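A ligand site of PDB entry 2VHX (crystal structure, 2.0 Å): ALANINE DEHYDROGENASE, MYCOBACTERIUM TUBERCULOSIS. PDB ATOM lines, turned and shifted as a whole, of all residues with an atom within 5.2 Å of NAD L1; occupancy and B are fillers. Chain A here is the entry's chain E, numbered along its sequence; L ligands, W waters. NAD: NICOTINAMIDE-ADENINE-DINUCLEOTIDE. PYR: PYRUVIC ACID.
OD1 of Asp 270 sits at hydrogen-bond distance from O2D of NAD L1 (2.5 Å).
The backbone NH (N) of Met 301 sits at hydrogen-bond distance from an oxygen (O7N) of NAD L1 (2.5 Å).
The side-chain carboxylate (OD1) of Asp 198 lies within hydrogen-bond range of an oxygen (O2B) of NAD L1 (2.6 Å).
An oxygen (O1N) of NAD L1 sits at hydrogen-bond distance from the side-chain hydroxyl (OG) of Ser 134.
The backbone NH (N) of Ala 179 sits at hydrogen-bond distance from an oxygen (O2N) of NAD L1, at 2.7 Å.
An oxygen (O3B) of NAD L1 sits at hydrogen-bond distance from the side-chain amino group of Lys 203 (2.9 Å).
The backbone carbonyl oxygen (O) of Val 298 sits at hydrogen-bond distance from a nitrogen (N7N) of NAD L1 (3.0 Å).
O2A of NAD L1 sits at hydrogen-bond distance from N of Thr 178 (3.1 Å).
O of Ile 267 sits close to N7N of NAD L1 (3.3 Å).
The side-chain hydroxyl of Ser 220 sits close to a nitrogen (N1A) of NAD L1.
The backbone NH of Leu 240 sits at hydrogen-bond distance from an oxygen (O4B) of NAD L1, at 3.3 Å.
A ring nitrogen (NE2) of His 96 sits at hydrogen-bond distance from an oxygen (O3) of PYR L2, at 3.4 Å.
Water W4 lies within hydrogen-bond range of an oxygen (O2A) of NAD L1 and the side-chain amino group (NZ) of Lys 203.
Water W6 lies within hydrogen-bond range of O1N of NAD L1 (2.7 Å) and OG1 of Thr 178 (2.8 Å).
Water W1 bridges O2D of NAD L1 and OE1 of Gln 271.
Water W9 lies within hydrogen-bond range of O of Val 239 (2.7 Å) and O3D of NAD L1 (3.0 Å).
Water W8 lies within hydrogen-bond range of ND2 of Asn 200 (2.8 Å), NZ of Lys 203 (2.8 Å) and O2B of NAD L1 (3.1 Å).
Water W7 bridges OG of Ser 220 (3.0 Å) and N1A of NAD L1 (3.1 Å).
An oxygen (O7N) of NAD L1 sits close to the backbone carbonyl oxygen (O) of Ala 299, at 3.4 Å.
Leu 130 touches NAD L1 (CD1 to O2D, 3.7 Å).
Met 133 touches NAD L1.
CB of Ala 137 touches C4N of NAD L1, at 3.6 Å.
Gly 175 touches NAD L1 (CA to O4B, 3.98 Å).
Gly 177 touches NAD L1.
Ile 199 touches NAD L1.
Asn 200 touches NAD L1 (CB to O2B, 3.9 Å).
Ala 238 touches NAD L1.
Val 239 touches NAD L1.
Leu 249 touches NAD L1.
Ala 268 touches NAD L1 (CA to O3D, 3.8 Å).
CG of Gln 271 touches O3D of NAD L1, at 3.7 Å.
C of Asn 300 touches O7N of NAD L1, 3.4 Å away.
CD of Pro 302 touches O7N of NAD L1, 3.2 Å away.
Hydrophobic or aromatic side chains that line NAD L1: Leu 130, Met 133, Ala 137, Ala 179, Ile 199, Val 239, Leu 240, Leu 249, Ile 267, Met 301 and Pro 302.
Of the 36 residues printed, 26 come within 4 Å of NAD L1.
The nearest printed residue that does not touch NAD L1 is Ile 269 (4.1 Å).
O of Asp 198 is in hydrogen-bond range of N of Ser 220 (3.0 Å).
The backbone NH (N) of Asn 200 is in hydrogen-bond range of the side-chain carboxylate (OD1) of Asp 198 (2.8 Å).
The side-chain carboxylate (OD2) of Asp 198 sits at hydrogen-bond distance from the backbone NH (N) of Ala 176, 2.9 Å away.
The backbone carbonyl oxygen (O) of Leu 130 lies within hydrogen-bond range of the side-chain hydroxyl (OG) of Ser 134 (3.3 Å).
N of Lys 203 is in hydrogen-bond range of OD1 of Asn 200.
N of Val 239 lies within hydrogen-bond range of O of Ile 174, 3.4 Å away.
ND1 of His 96 lies within hydrogen-bond range of OE1 of Gln 271 (2.8 Å).
N of Gly 175 sits at hydrogen-bond distance from O of Leu 197 (2.7 Å).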
ATOM      1  N   HIS A  96      36.838  27.172 -26.504  1.00  0.00           N
ATOM      2  CA  HIS A  96      36.854  27.543 -25.091  1.00  0.00           C
ATOM      3  C   HIS A  96      38.037  28.483 -24.730  1.00  0.00           C
ATOM      4  O   HIS A  96      38.683  28.310 -23.686  1.00  0.00           O
ATOM      5  CB  HIS A  96      36.886  26.278 -24.226  1.00  0.00           C
ATOM      6  CG  HIS A  96      35.880  25.243 -24.610  1.00  0.00           C
ATOM      7  ND1 HIS A  96      34.521  25.438 -24.487  1.00  0.00           N
ATOM      8  CD2 HIS A  96      36.039  23.981 -25.091  1.00  0.00           C
ATOM      9  CE1 HIS A  96      33.882  24.353 -24.893  1.00  0.00           C
ATOM     10  NE2 HIS A  96      34.778  23.459 -25.261  1.00  0.00           N
ATOM     11  N   LEU A 127      22.582  28.899 -28.967  1.00  0.00           N
ATOM     12  CA  LEU A 127      23.911  28.461 -29.406  1.00  0.00           C
ATOM     13  C   LEU A 127      23.737  27.077 -30.036  1.00  0.00           C
ATOM     14  O   LEU A 127      23.858  26.061 -29.361  1.00  0.00           O
ATOM     15  CB  LEU A 127      24.877  28.413 -28.214  1.00  0.00           C
ATOM     16  CG  LEU A 127      25.107  29.754 -27.486  1.00  0.00           C
ATOM     17  CD1 LEU A 127      25.685  29.579 -26.069  1.00  0.00           C
ATOM     18  CD2 LEU A 127      25.985  30.678 -28.308  1.00  0.00           C
ATOM     19  N   LEU A 130      26.791  24.396 -29.674  1.00  0.00           N
ATOM     20  CA  LEU A 130      26.977  23.955 -28.296  1.00  0.00           C
ATOM     21  C   LEU A 130      25.794  23.091 -27.805  1.00  0.00           C
ATOM     22  O   LEU A 130      26.009  22.127 -27.075  1.00  0.00           O
ATOM     23  CB  LEU A 130      27.187  25.155 -27.357  1.00  0.00           C
ATOM     24  CG  LEU A 130      27.407  24.858 -25.866  1.00  0.00           C
ATOM     25  CD1 LEU A 130      28.699  24.091 -25.634  1.00  0.00           C
ATOM     26  CD2 LEU A 130      27.464  26.161 -25.121  1.00  0.00           C
ATOM     27  N   MET A 133      25.844  19.191 -27.643  1.00  0.00           N
ATOM     28  CA  MET A 133      26.853  18.720 -26.674  1.00  0.00           C
ATOM     29  C   MET A 133      26.441  19.014 -25.233  1.00  0.00           C
ATOM     30  O   MET A 133      26.694  18.208 -24.337  1.00  0.00           O
ATOM     31  CB  MET A 133      28.219  19.285 -27.005  1.00  0.00           C
ATOM     32  CG  MET A 133      28.790  18.772 -28.351  1.00  0.00           C
ATOM     33  SD  MET A 133      28.791  16.980 -28.546  1.00  0.00           S
ATOM     34  CE  MET A 133      27.145  16.664 -29.217  1.00  0.00           C
ATOM     35  N   SER A 134      25.773  20.126 -24.998  1.00  0.00           N
ATOM     36  CA  SER A 134      25.268  20.400 -23.664  1.00  0.00           C
ATOM     37  C   SER A 134      24.137  19.415 -23.336  1.00  0.00           C
ATOM     38  O   SER A 134      23.939  19.044 -22.188  1.00  0.00           O
ATOM     39  CB  SER A 134      24.681  21.795 -23.607  1.00  0.00           C
ATOM     40  OG  SER A 134      25.663  22.745 -23.883  1.00  0.00           O
ATOM     41  N   ALA A 137      26.130  16.275 -22.322  1.00  0.00           N
ATOM     42  CA  ALA A 137      26.883  16.460 -21.089  1.00  0.00           C
ATOM     43  C   ALA A 137      25.905  16.472 -19.935  1.00  0.00           C
ATOM     44  O   ALA A 137      26.171  15.865 -18.894  1.00  0.00           O
ATOM     45  CB  ALA A 137      27.668  17.746 -21.150  1.00  0.00           C
ATOM     46  N   ILE A 174      22.732  23.933 -10.861  1.00  0.00           N
ATOM     47  CA  ILE A 174      22.923  25.385 -11.008  1.00  0.00           C
ATOM     48  C   ILE A 174      22.963  25.760 -12.490  1.00  0.00           C
ATOM     49  O   ILE A 174      23.920  25.386 -13.194  1.00  0.00           O
ATOM     50  CB  ILE A 174      24.197  25.846 -10.264  1.00  0.00           C
ATOM     51  CG1 ILE A 174      24.235  25.250  -8.837  1.00  0.00           C
ATOM     52  CG2 ILE A 174      24.242  27.388 -10.203  1.00  0.00           C
ATOM     53  CD1 ILE A 174      25.592  25.428  -8.136  1.00  0.00           C
ATOM     54  N   GLY A 175      21.938  26.445 -12.971  1.00  0.00           N
ATOM     55  CA  GLY A 175      21.783  26.681 -14.415  1.00  0.00           C
ATOM     56  C   GLY A 175      20.627  25.888 -14.965  1.00  0.00           C
ATOM     57  O   GLY A 175      20.615  24.660 -14.862  1.00  0.00           O
ATOM     58  N   ALA A 176      19.683  26.568 -15.618  1.00  0.00           N
ATOM     59  CA  ALA A 176      18.488  25.962 -16.193  1.00  0.00           C
ATOM     60  C   ALA A 176      18.458  26.075 -17.738  1.00  0.00           C
ATOM     61  O   ALA A 176      17.390  26.051 -18.339  1.00  0.00           O
ATOM     62  CB  ALA A 176      17.198  26.626 -15.579  1.00  0.00           C
ATOM     63  N   GLY A 177      19.615  26.230 -18.363  1.00  0.00           N
ATOM     64  CA  GLY A 177      19.699  26.206 -19.814  1.00  0.00           C
ATOM     65  C   GLY A 177      19.802  24.765 -20.323  1.00  0.00           C
ATOM     66  O   GLY A 177      19.297  23.837 -19.693  1.00  0.00           O
ATOM     67  N   THR A 178      20.441  24.579 -21.465  1.00  0.00           N
ATOM     68  CA  THR A 178      20.452  23.244 -22.071  1.00  0.00           C
ATOM     69  C   THR A 178      21.051  22.145 -21.174  1.00  0.00           C
ATOM     70  O   THR A 178      20.449  21.080 -21.036  1.00  0.00           O
ATOM     71  CB  THR A 178      21.136  23.236 -23.470  1.00  0.00           C
ATOM     72  OG1 THR A 178      20.580  24.295 -24.270  1.00  0.00           O
ATOM     73  CG2 THR A 178      20.937  21.905 -24.195  1.00  0.00           C
ATOM     74  N   ALA A 179      22.192  22.416 -20.549  1.00  0.00           N
ATOM     75  CA  ALA A 179      22.859  21.382 -19.817  1.00  0.00           C
ATOM     76  C   ALA A 179      22.069  21.085 -18.559  1.00  0.00           C
ATOM     77  O   ALA A 179      21.847  19.904 -18.245  1.00  0.00           O
ATOM     78  CB  ALA A 179      24.324  21.773 -19.497  1.00  0.00           C
ATOM     79  N   GLY A 180      21.643  22.139 -17.860  1.00  0.00           N
ATOM     80  CA  GLY A 180      20.994  22.024 -16.556  1.00  0.00           C
ATOM     81  C   GLY A 180      19.635  21.389 -16.651  1.00  0.00           C
ATOM     82  O   GLY A 180      19.257  20.594 -15.801  1.00  0.00           O
ATOM     83  N   LEU A 197      18.419  26.082  -9.933  1.00  0.00           N
ATOM     84  CA  LEU A 197      18.572  27.516  -9.736  1.00  0.00           C
ATOM     85  C   LEU A 197      19.005  28.162 -11.026  1.00  0.00           C
ATOM     86  O   LEU A 197      19.839  27.626 -11.769  1.00  0.00           O
ATOM     87  CB  LEU A 197      19.653  27.823  -8.679  1.00  0.00           C
ATOM     88  CG  LEU A 197      19.791  27.419  -7.211  1.00  0.00           C
ATOM     89  CD1 LEU A 197      19.341  28.540  -6.279  1.00  0.00           C
ATOM     90  CD2 LEU A 197      19.111  26.164  -6.856  1.00  0.00           C
ATOM     91  N   ASP A 198      18.478  29.357 -11.276  1.00  0.00           N
ATOM     92  CA  ASP A 198      18.949  30.195 -12.339  1.00  0.00           C
ATOM     93  C   ASP A 198      18.596  31.658 -12.001  1.00  0.00           C
ATOM     94  O   ASP A 198      17.725  31.917 -11.167  1.00  0.00           O
ATOM     95  CB  ASP A 198      18.329  29.747 -13.674  1.00  0.00           C
ATOM     96  CG  ASP A 198      19.108  30.253 -14.897  1.00  0.00           C
ATOM     97  OD1 ASP A 198      19.369  31.485 -15.034  1.00  0.00           O
ATOM     98  OD2 ASP A 198      19.414  29.421 -15.761  1.00  0.00           O
ATOM     99  N   ILE A 199      19.290  32.602 -12.632  1.00  0.00           N
ATOM    100  CA  ILE A 199      18.965  34.014 -12.476  1.00  0.00           C
ATOM    101  C   ILE A 199      17.912  34.463 -13.489  1.00  0.00           C
ATOM    102  O   ILE A 199      17.339  35.549 -13.357  1.00  0.00           O
ATOM    103  CB  ILE A 199      20.220  34.895 -12.568  1.00  0.00           C
ATOM    104  CG1 ILE A 199      20.968  34.668 -13.878  1.00  0.00           C
ATOM    105  CG2 ILE A 199      21.147  34.607 -11.367  1.00  0.00           C
ATOM    106  CD1 ILE A 199      22.042  35.752 -14.194  1.00  0.00           C
ATOM    107  N   ASN A 200      17.643  33.614 -14.485  1.00  0.00           N
ATOM    108  CA  ASN A 200      16.651  33.901 -15.535  1.00  0.00           C
ATOM    109  C   ASN A 200      15.367  33.164 -15.144  1.00  0.00           C
ATOM    110  O   ASN A 200      15.268  31.932 -15.319  1.00  0.00           O
ATOM    111  CB  ASN A 200      17.183  33.381 -16.873  1.00  0.00           C
ATOM    112  CG  ASN A 200      16.210  33.618 -18.041  1.00  0.00           C
ATOM    113  OD1 ASN A 200      15.003  33.731 -17.846  1.00  0.00           O
ATOM    114  ND2 ASN A 200      16.744  33.650 -19.255  1.00  0.00           N
ATOM    115  N   LYS A 203      13.461  30.749 -17.657  1.00  0.00           N
ATOM    116  CA  LYS A 203      13.960  29.396 -17.691  1.00  0.00           C
ATOM    117  C   LYS A 203      13.377  28.532 -16.560  1.00  0.00           C
ATOM    118  O   LYS A 203      13.089  27.324 -16.755  1.00  0.00           O
ATOM    119  CB  LYS A 203      15.487  29.434 -17.707  1.00  0.00           C
ATOM    120  CG  LYS A 203      15.962  29.797 -19.116  1.00  0.00           C
ATOM    121  CD  LYS A 203      17.442  29.851 -19.235  1.00  0.00           C
ATOM    122  CE  LYS A 203      17.814  29.959 -20.724  1.00  0.00           C
ATOM    123  NZ  LYS A 203      19.250  30.334 -20.952  1.00  0.00           N
ATOM    124  N   SER A 220      18.303  32.184  -8.252  1.00  0.00           N
ATOM    125  CA  SER A 220      19.659  31.899  -7.841  1.00  0.00           C
ATOM    126  C   SER A 220      20.331  33.118  -7.276  1.00  0.00           C
ATOM    127  O   SER A 220      20.887  33.886  -8.024  1.00  0.00           O
ATOM    128  CB  SER A 220      20.493  31.467  -9.025  1.00  0.00           C
ATOM    129  OG  SER A 220      21.757  31.033  -8.588  1.00  0.00           O
ATOM    130  N   ALA A 238      26.227  24.053 -14.111  1.00  0.00           N
ATOM    131  CA  ALA A 238      25.809  24.057 -15.499  1.00  0.00           C
ATOM    132  C   ALA A 238      25.511  25.473 -15.990  1.00  0.00           C
ATOM    133  O   ALA A 238      24.598  25.692 -16.793  1.00  0.00           O
ATOM    134  CB  ALA A 238      24.586  23.204 -15.642  1.00  0.00           C
ATOM    135  N   VAL A 239      26.247  26.445 -15.482  1.00  0.00           N
ATOM    136  CA  VAL A 239      26.007  27.844 -15.843  1.00  0.00           C
ATOM    137  C   VAL A 239      26.899  28.248 -17.001  1.00  0.00           C
ATOM    138  O   VAL A 239      27.950  27.661 -17.193  1.00  0.00           O
ATOM    139  CB  VAL A 239      26.328  28.800 -14.667  1.00  0.00           C
ATOM    140  CG1 VAL A 239      25.478  28.463 -13.425  1.00  0.00           C
ATOM    141  CG2 VAL A 239      27.809  28.710 -14.324  1.00  0.00           C
ATOM    142  N   LEU A 240      26.467  29.243 -17.756  1.00  0.00           N
ATOM    143  CA  LEU A 240      27.194  29.770 -18.888  1.00  0.00           C
ATOM    144  C   LEU A 240      26.904  31.249 -19.066  1.00  0.00           C
ATOM    145  O   LEU A 240      25.750  31.708 -18.943  1.00  0.00           O
ATOM    146  CB  LEU A 240      26.759  29.063 -20.162  1.00  0.00           C
ATOM    147  CG  LEU A 240      27.626  28.891 -21.436  1.00  0.00           C
ATOM    148  CD1 LEU A 240      26.853  29.094 -22.679  1.00  0.00           C
ATOM    149  CD2 LEU A 240      28.950  29.623 -21.446  1.00  0.00           C
ATOM    150  N   VAL A 241      27.968  31.999 -19.335  1.00  0.00           N
ATOM    151  CA  VAL A 241      27.849  33.269 -20.042  1.00  0.00           C
ATOM    152  C   VAL A 241      28.610  33.085 -21.363  1.00  0.00           C
ATOM    153  O   VAL A 241      29.818  32.875 -21.333  1.00  0.00           O
ATOM    154  CB  VAL A 241      28.446  34.403 -19.203  1.00  0.00           C
ATOM    155  CG1 VAL A 241      28.324  35.737 -19.937  1.00  0.00           C
ATOM    156  CG2 VAL A 241      27.774  34.465 -17.838  1.00  0.00           C
ATOM    157  N   PRO A 247      31.572  31.980 -13.897  1.00  0.00           N
ATOM    158  CA  PRO A 247      31.749  32.636 -12.602  1.00  0.00           C
ATOM    159  C   PRO A 247      31.943  31.548 -11.531  1.00  0.00           C
ATOM    160  O   PRO A 247      31.385  30.438 -11.673  1.00  0.00           O
ATOM    161  CB  PRO A 247      30.425  33.372 -12.400  1.00  0.00           C
ATOM    162  CG  PRO A 247      29.430  32.522 -13.150  1.00  0.00           C
ATOM    163  CD  PRO A 247      30.173  32.004 -14.360  1.00  0.00           C
ATOM    164  N   LEU A 249      30.912  30.107  -8.420  1.00  0.00           N
ATOM    165  CA  LEU A 249      29.677  30.252  -7.661  1.00  0.00           C
ATOM    166  C   LEU A 249      29.661  29.456  -6.364  1.00  0.00           C
ATOM    167  O   LEU A 249      28.954  29.813  -5.426  1.00  0.00           O
ATOM    168  CB  LEU A 249      28.467  29.861  -8.522  1.00  0.00           C
ATOM    169  CG  LEU A 249      28.148  30.757  -9.724  1.00  0.00           C
ATOM    170  CD1 LEU A 249      26.874  30.319 -10.330  1.00  0.00           C
ATOM    171  CD2 LEU A 249      28.026  32.222  -9.351  1.00  0.00           C
ATOM    172  N   ASP A 266      31.077  19.440 -12.232  1.00  0.00           N
ATOM    173  CA  ASP A 266      31.178  20.759 -12.798  1.00  0.00           C
ATOM    174  C   ASP A 266      31.158  20.638 -14.317  1.00  0.00           C
ATOM    175  O   ASP A 266      32.219  20.495 -14.934  1.00  0.00           O
ATOM    176  CB  ASP A 266      32.476  21.412 -12.348  1.00  0.00           C
ATOM    177  CG  ASP A 266      32.457  22.938 -12.491  1.00  0.00           C
ATOM    178  OD1 ASP A 266      31.586  23.493 -13.201  1.00  0.00           O
ATOM    179  OD2 ASP A 266      33.339  23.603 -11.892  1.00  0.00           O
ATOM    180  N   ILE A 267      29.977  20.707 -14.937  1.00  0.00           N
ATOM    181  CA  ILE A 267      29.876  20.713 -16.387  1.00  0.00           C
ATOM    182  C   ILE A 267      30.576  21.970 -16.980  1.00  0.00           C
ATOM    183  O   ILE A 267      31.155  21.892 -18.078  1.00  0.00           O
ATOM    184  CB  ILE A 267      28.400  20.594 -16.869  1.00  0.00           C
ATOM    185  CG1 ILE A 267      27.679  19.415 -16.196  1.00  0.00           C
ATOM    186  CG2 ILE A 267      28.326  20.396 -18.398  1.00  0.00           C
ATOM    187  CD1 ILE A 267      26.202  19.402 -16.544  1.00  0.00           C
ATOM    188  N   ALA A 268      30.550  23.101 -16.268  1.00  0.00           N
ATOM    189  CA  ALA A 268      31.148  24.355 -16.773  1.00  0.00           C
ATOM    190  C   ALA A 268      32.697  24.361 -16.738  1.00  0.00           C
ATOM    191  O   ALA A 268      33.343  25.375 -17.018  1.00  0.00           O
ATOM    192  CB  ALA A 268      30.582  25.545 -16.035  1.00  0.00           C
ATOM    193  N   ILE A 269      33.299  23.227 -16.387  1.00  0.00           N
ATOM    194  CA  ILE A 269      34.760  23.097 -16.389  1.00  0.00           C
ATOM    195  C   ILE A 269      35.392  23.471 -17.739  1.00  0.00           C
ATOM    196  O   ILE A 269      36.495  24.037 -17.778  1.00  0.00           O
ATOM    197  CB  ILE A 269      35.240  21.686 -15.928  1.00  0.00           C
ATOM    198  CG1 ILE A 269      36.762  21.625 -15.769  1.00  0.00           C
ATOM    199  CG2 ILE A 269      34.780  20.636 -16.912  1.00  0.00           C
ATOM    200  CD1 ILE A 269      37.326  22.685 -14.828  1.00  0.00           C
ATOM    201  N   ASP A 270      34.689  23.213 -18.835  1.00  0.00           N
ATOM    202  CA  ASP A 270      35.210  23.563 -20.171  1.00  0.00           C
ATOM    203  C   ASP A 270      35.455  25.072 -20.331  1.00  0.00           C
ATOM    204  O   ASP A 270      36.311  25.467 -21.100  1.00  0.00           O
ATOM    205  CB  ASP A 270      34.310  23.031 -21.286  1.00  0.00           C
ATOM    206  CG  ASP A 270      32.920  23.718 -21.326  1.00  0.00           C
ATOM    207  OD1 ASP A 270      32.289  23.669 -22.407  1.00  0.00           O
ATOM    208  OD2 ASP A 270      32.446  24.289 -20.309  1.00  0.00           O
ATOM    209  N   GLN A 271      34.705  25.878 -19.599  1.00  0.00           N
ATOM    210  CA  GLN A 271      34.907  27.338 -19.543  1.00  0.00           C
ATOM    211  C   GLN A 271      35.586  27.754 -18.264  1.00  0.00           C
ATOM    212  O   GLN A 271      35.502  28.918 -17.864  1.00  0.00           O
ATOM    213  CB  GLN A 271      33.579  28.083 -19.715  1.00  0.00           C
ATOM    214  CG  GLN A 271      32.877  27.852 -21.070  1.00  0.00           C
ATOM    215  CD  GLN A 271      33.607  28.438 -22.278  1.00  0.00           C
ATOM    216  OE1 GLN A 271      33.647  27.809 -23.348  1.00  0.00           O
ATOM    217  NE2 GLN A 271      34.134  29.658 -22.135  1.00  0.00           N
ATOM    218  N   VAL A 298      35.294  16.767 -15.931  1.00  0.00           N
ATOM    219  CA  VAL A 298      35.771  16.288 -17.221  1.00  0.00           C
ATOM    220  C   VAL A 298      35.293  17.291 -18.255  1.00  0.00           C
ATOM    221  O   VAL A 298      34.067  17.580 -18.337  1.00  0.00           O
ATOM    222  CB  VAL A 298      35.260  14.854 -17.538  1.00  0.00           C
ATOM    223  CG1 VAL A 298      35.649  14.438 -18.929  1.00  0.00           C
ATOM    224  CG2 VAL A 298      35.840  13.871 -16.516  1.00  0.00           C
ATOM    225  N   ALA A 299      36.238  17.837 -19.025  1.00  0.00           N
ATOM    226  CA  ALA A 299      35.913  18.908 -19.982  1.00  0.00           C
ATOM    227  C   ALA A 299      35.515  18.405 -21.364  1.00  0.00           C
ATOM    228  O   ALA A 299      35.153  19.206 -22.222  1.00  0.00           O
ATOM    229  CB  ALA A 299      37.065  19.929 -20.080  1.00  0.00           C
ATOM    230  N   ASN A 300      35.583  17.095 -21.602  1.00  0.00           N
ATOM    231  CA  ASN A 300      35.054  16.505 -22.849  1.00  0.00           C
ATOM    232  C   ASN A 300      34.063  15.365 -22.583  1.00  0.00           C
ATOM    233  O   ASN A 300      34.200  14.261 -23.104  1.00  0.00           O
ATOM    234  CB  ASN A 300      36.197  16.042 -23.778  1.00  0.00           C
ATOM    235  CG  ASN A 300      36.993  14.867 -23.210  1.00  0.00           C
ATOM    236  OD1 ASN A 300      37.069  14.694 -21.985  1.00  0.00           O
ATOM    237  ND2 ASN A 300      37.594  14.064 -24.081  1.00  0.00           N
ATOM    238  N   MET A 301      33.029  15.665 -21.773  1.00  0.00           N
ATOM    239  CA  MET A 301      32.067  14.657 -21.332  1.00  0.00           C
ATOM    240  C   MET A 301      31.452  13.779 -22.476  1.00  0.00           C
ATOM    241  O   MET A 301      31.432  12.555 -22.361  1.00  0.00           O
ATOM    242  CB  MET A 301      30.983  15.274 -20.445  1.00  0.00           C
ATOM    243  CG  MET A 301      31.543  15.711 -19.070  1.00  0.00           C
ATOM    244  SD  MET A 301      30.346  16.570 -17.998  1.00  0.00           S
ATOM    245  CE  MET A 301      29.451  15.201 -17.260  1.00  0.00           C
ATOM    246  N   PRO A 302      30.976  14.407 -23.561  1.00  0.00           N
ATOM    247  CA  PRO A 302      30.279  13.607 -24.607  1.00  0.00           C
ATOM    248  C   PRO A 302      31.188  12.601 -25.366  1.00  0.00           C
ATOM    249  O   PRO A 302      30.695  11.813 -26.175  1.00  0.00           O
ATOM    250  CB  PRO A 302      29.769  14.695 -25.579  1.00  0.00           C
ATOM    251  CG  PRO A 302      29.790  15.983 -24.766  1.00  0.00           C
ATOM    252  CD  PRO A 302      31.023  15.833 -23.925  1.00  0.00           C
HETATM  253  PA  NAD L   1      22.951  27.802 -21.464  1.00  0.00           P
HETATM  254  O1A NAD L   1      23.203  29.167 -21.922  1.00  0.00           O
HETATM  255  O2A NAD L   1      21.883  27.174 -22.291  1.00  0.00           O
HETATM  256  O5B NAD L   1      22.544  27.918 -19.899  1.00  0.00           O
HETATM  257  C5B NAD L   1      23.408  28.546 -18.981  1.00  0.00           C
HETATM  258  C4B NAD L   1      22.495  29.081 -17.891  1.00  0.00           C
HETATM  259  O4B NAD L   1      23.274  29.500 -16.791  1.00  0.00           O
HETATM  260  C3B NAD L   1      21.638  30.237 -18.374  1.00  0.00           C
HETATM  261  O3B NAD L   1      20.268  29.898 -18.233  1.00  0.00           O
HETATM  262  C2B NAD L   1      21.994  31.360 -17.405  1.00  0.00           C
HETATM  263  O2B NAD L   1      20.896  32.187 -17.034  1.00  0.00           O
HETATM  264  C1B NAD L   1      22.557  30.572 -16.232  1.00  0.00           C
HETATM  265  N9A NAD L   1      23.412  31.372 -15.365  1.00  0.00           N
HETATM  266  C8A NAD L   1      24.432  32.195 -15.759  1.00  0.00           C
HETATM  267  N7A NAD L   1      24.978  32.730 -14.636  1.00  0.00           N
HETATM  268  C5A NAD L   1      24.337  32.278 -13.560  1.00  0.00           C
HETATM  269  C6A NAD L   1      24.511  32.545 -12.200  1.00  0.00           C
HETATM  270  N6A NAD L   1      25.466  33.401 -11.832  1.00  0.00           N
HETATM  271  N1A NAD L   1      23.689  31.901 -11.277  1.00  0.00           N
HETATM  272  C2A NAD L   1      22.709  31.015 -11.736  1.00  0.00           C
HETATM  273  N3A NAD L   1      22.549  30.775 -13.093  1.00  0.00           N
HETATM  274  C4A NAD L   1      23.341  31.404 -13.988  1.00  0.00           C
HETATM  275  O3  NAD L   1      24.304  26.997 -21.519  1.00  0.00           O
HETATM  276  PN  NAD L   1      24.482  25.415 -21.666  1.00  0.00           P
HETATM  277  O1N NAD L   1      24.500  24.991 -23.102  1.00  0.00           O
HETATM  278  O2N NAD L   1      23.566  24.752 -20.682  1.00  0.00           O
HETATM  279  O5D NAD L   1      25.974  25.166 -21.164  1.00  0.00           O
HETATM  280  C5D NAD L   1      26.337  25.060 -19.817  1.00  0.00           C
HETATM  281  C4D NAD L   1      27.831  24.789 -19.676  1.00  0.00           C
HETATM  282  O4D NAD L   1      28.066  23.415 -19.963  1.00  0.00           O
HETATM  283  C3D NAD L   1      28.695  25.611 -20.634  1.00  0.00           C
HETATM  284  O3D NAD L   1      29.902  25.996 -20.017  1.00  0.00           O
HETATM  285  C2D NAD L   1      29.030  24.591 -21.669  1.00  0.00           C
HETATM  286  O2D NAD L   1      30.184  24.941 -22.394  1.00  0.00           O
HETATM  287  C1D NAD L   1      29.206  23.355 -20.786  1.00  0.00           C
HETATM  288  N1N NAD L   1      29.426  22.116 -21.551  1.00  0.00           N
HETATM  289  C2N NAD L   1      30.444  21.315 -21.117  1.00  0.00           C
HETATM  290  C3N NAD L   1      30.760  20.136 -21.782  1.00  0.00           C
HETATM  291  C7N NAD L   1      31.684  19.151 -21.107  1.00  0.00           C
HETATM  292  O7N NAD L   1      31.968  17.962 -21.775  1.00  0.00           O
HETATM  293  N7N NAD L   1      32.175  19.396 -19.894  1.00  0.00           N
HETATM  294  C4N NAD L   1      30.011  19.755 -22.916  1.00  0.00           C
HETATM  295  C5N NAD L   1      28.953  20.585 -23.333  1.00  0.00           C
HETATM  296  C6N NAD L   1      28.670  21.770 -22.636  1.00  0.00           C
HETATM  297  C   PYR L   2      32.336  18.970 -25.629  1.00  0.00           C
HETATM  298  O   PYR L   2      33.425  18.298 -25.464  1.00  0.00           O
HETATM  299  OXT PYR L   2      31.414  18.494 -26.396  1.00  0.00           O
HETATM  300  CA  PYR L   2      32.214  20.174 -24.997  1.00  0.00           C
HETATM  301  O3  PYR L   2      33.162  20.600 -24.242  1.00  0.00           O
HETATM  302  CB  PYR L   2      31.010  21.045 -25.138  1.00  0.00           C
HETATM  303  O   HOH W   1      30.905  27.080 -24.069  1.00  0.00           O
HETATM  304  O   HOH W   2      22.502  24.917 -18.356  1.00  0.00           O
HETATM  305  O   HOH W   3      23.749  31.651 -21.050  1.00  0.00           O
HETATM  306  O   HOH W   4      19.513  28.029 -22.694  1.00  0.00           O
HETATM  307  O   HOH W   5      26.574  34.996 -14.541  1.00  0.00           O
HETATM  308  O   HOH W   6      22.819  25.656 -25.158  1.00  0.00           O
HETATM  309  O   HOH W   7      24.050  32.993  -8.400  1.00  0.00           O
HETATM  310  O   HOH W   8      19.352  32.830 -19.629  1.00  0.00           O
HETATM  311  O   HOH W   9      30.350  28.365 -18.298  1.00  0.00           O
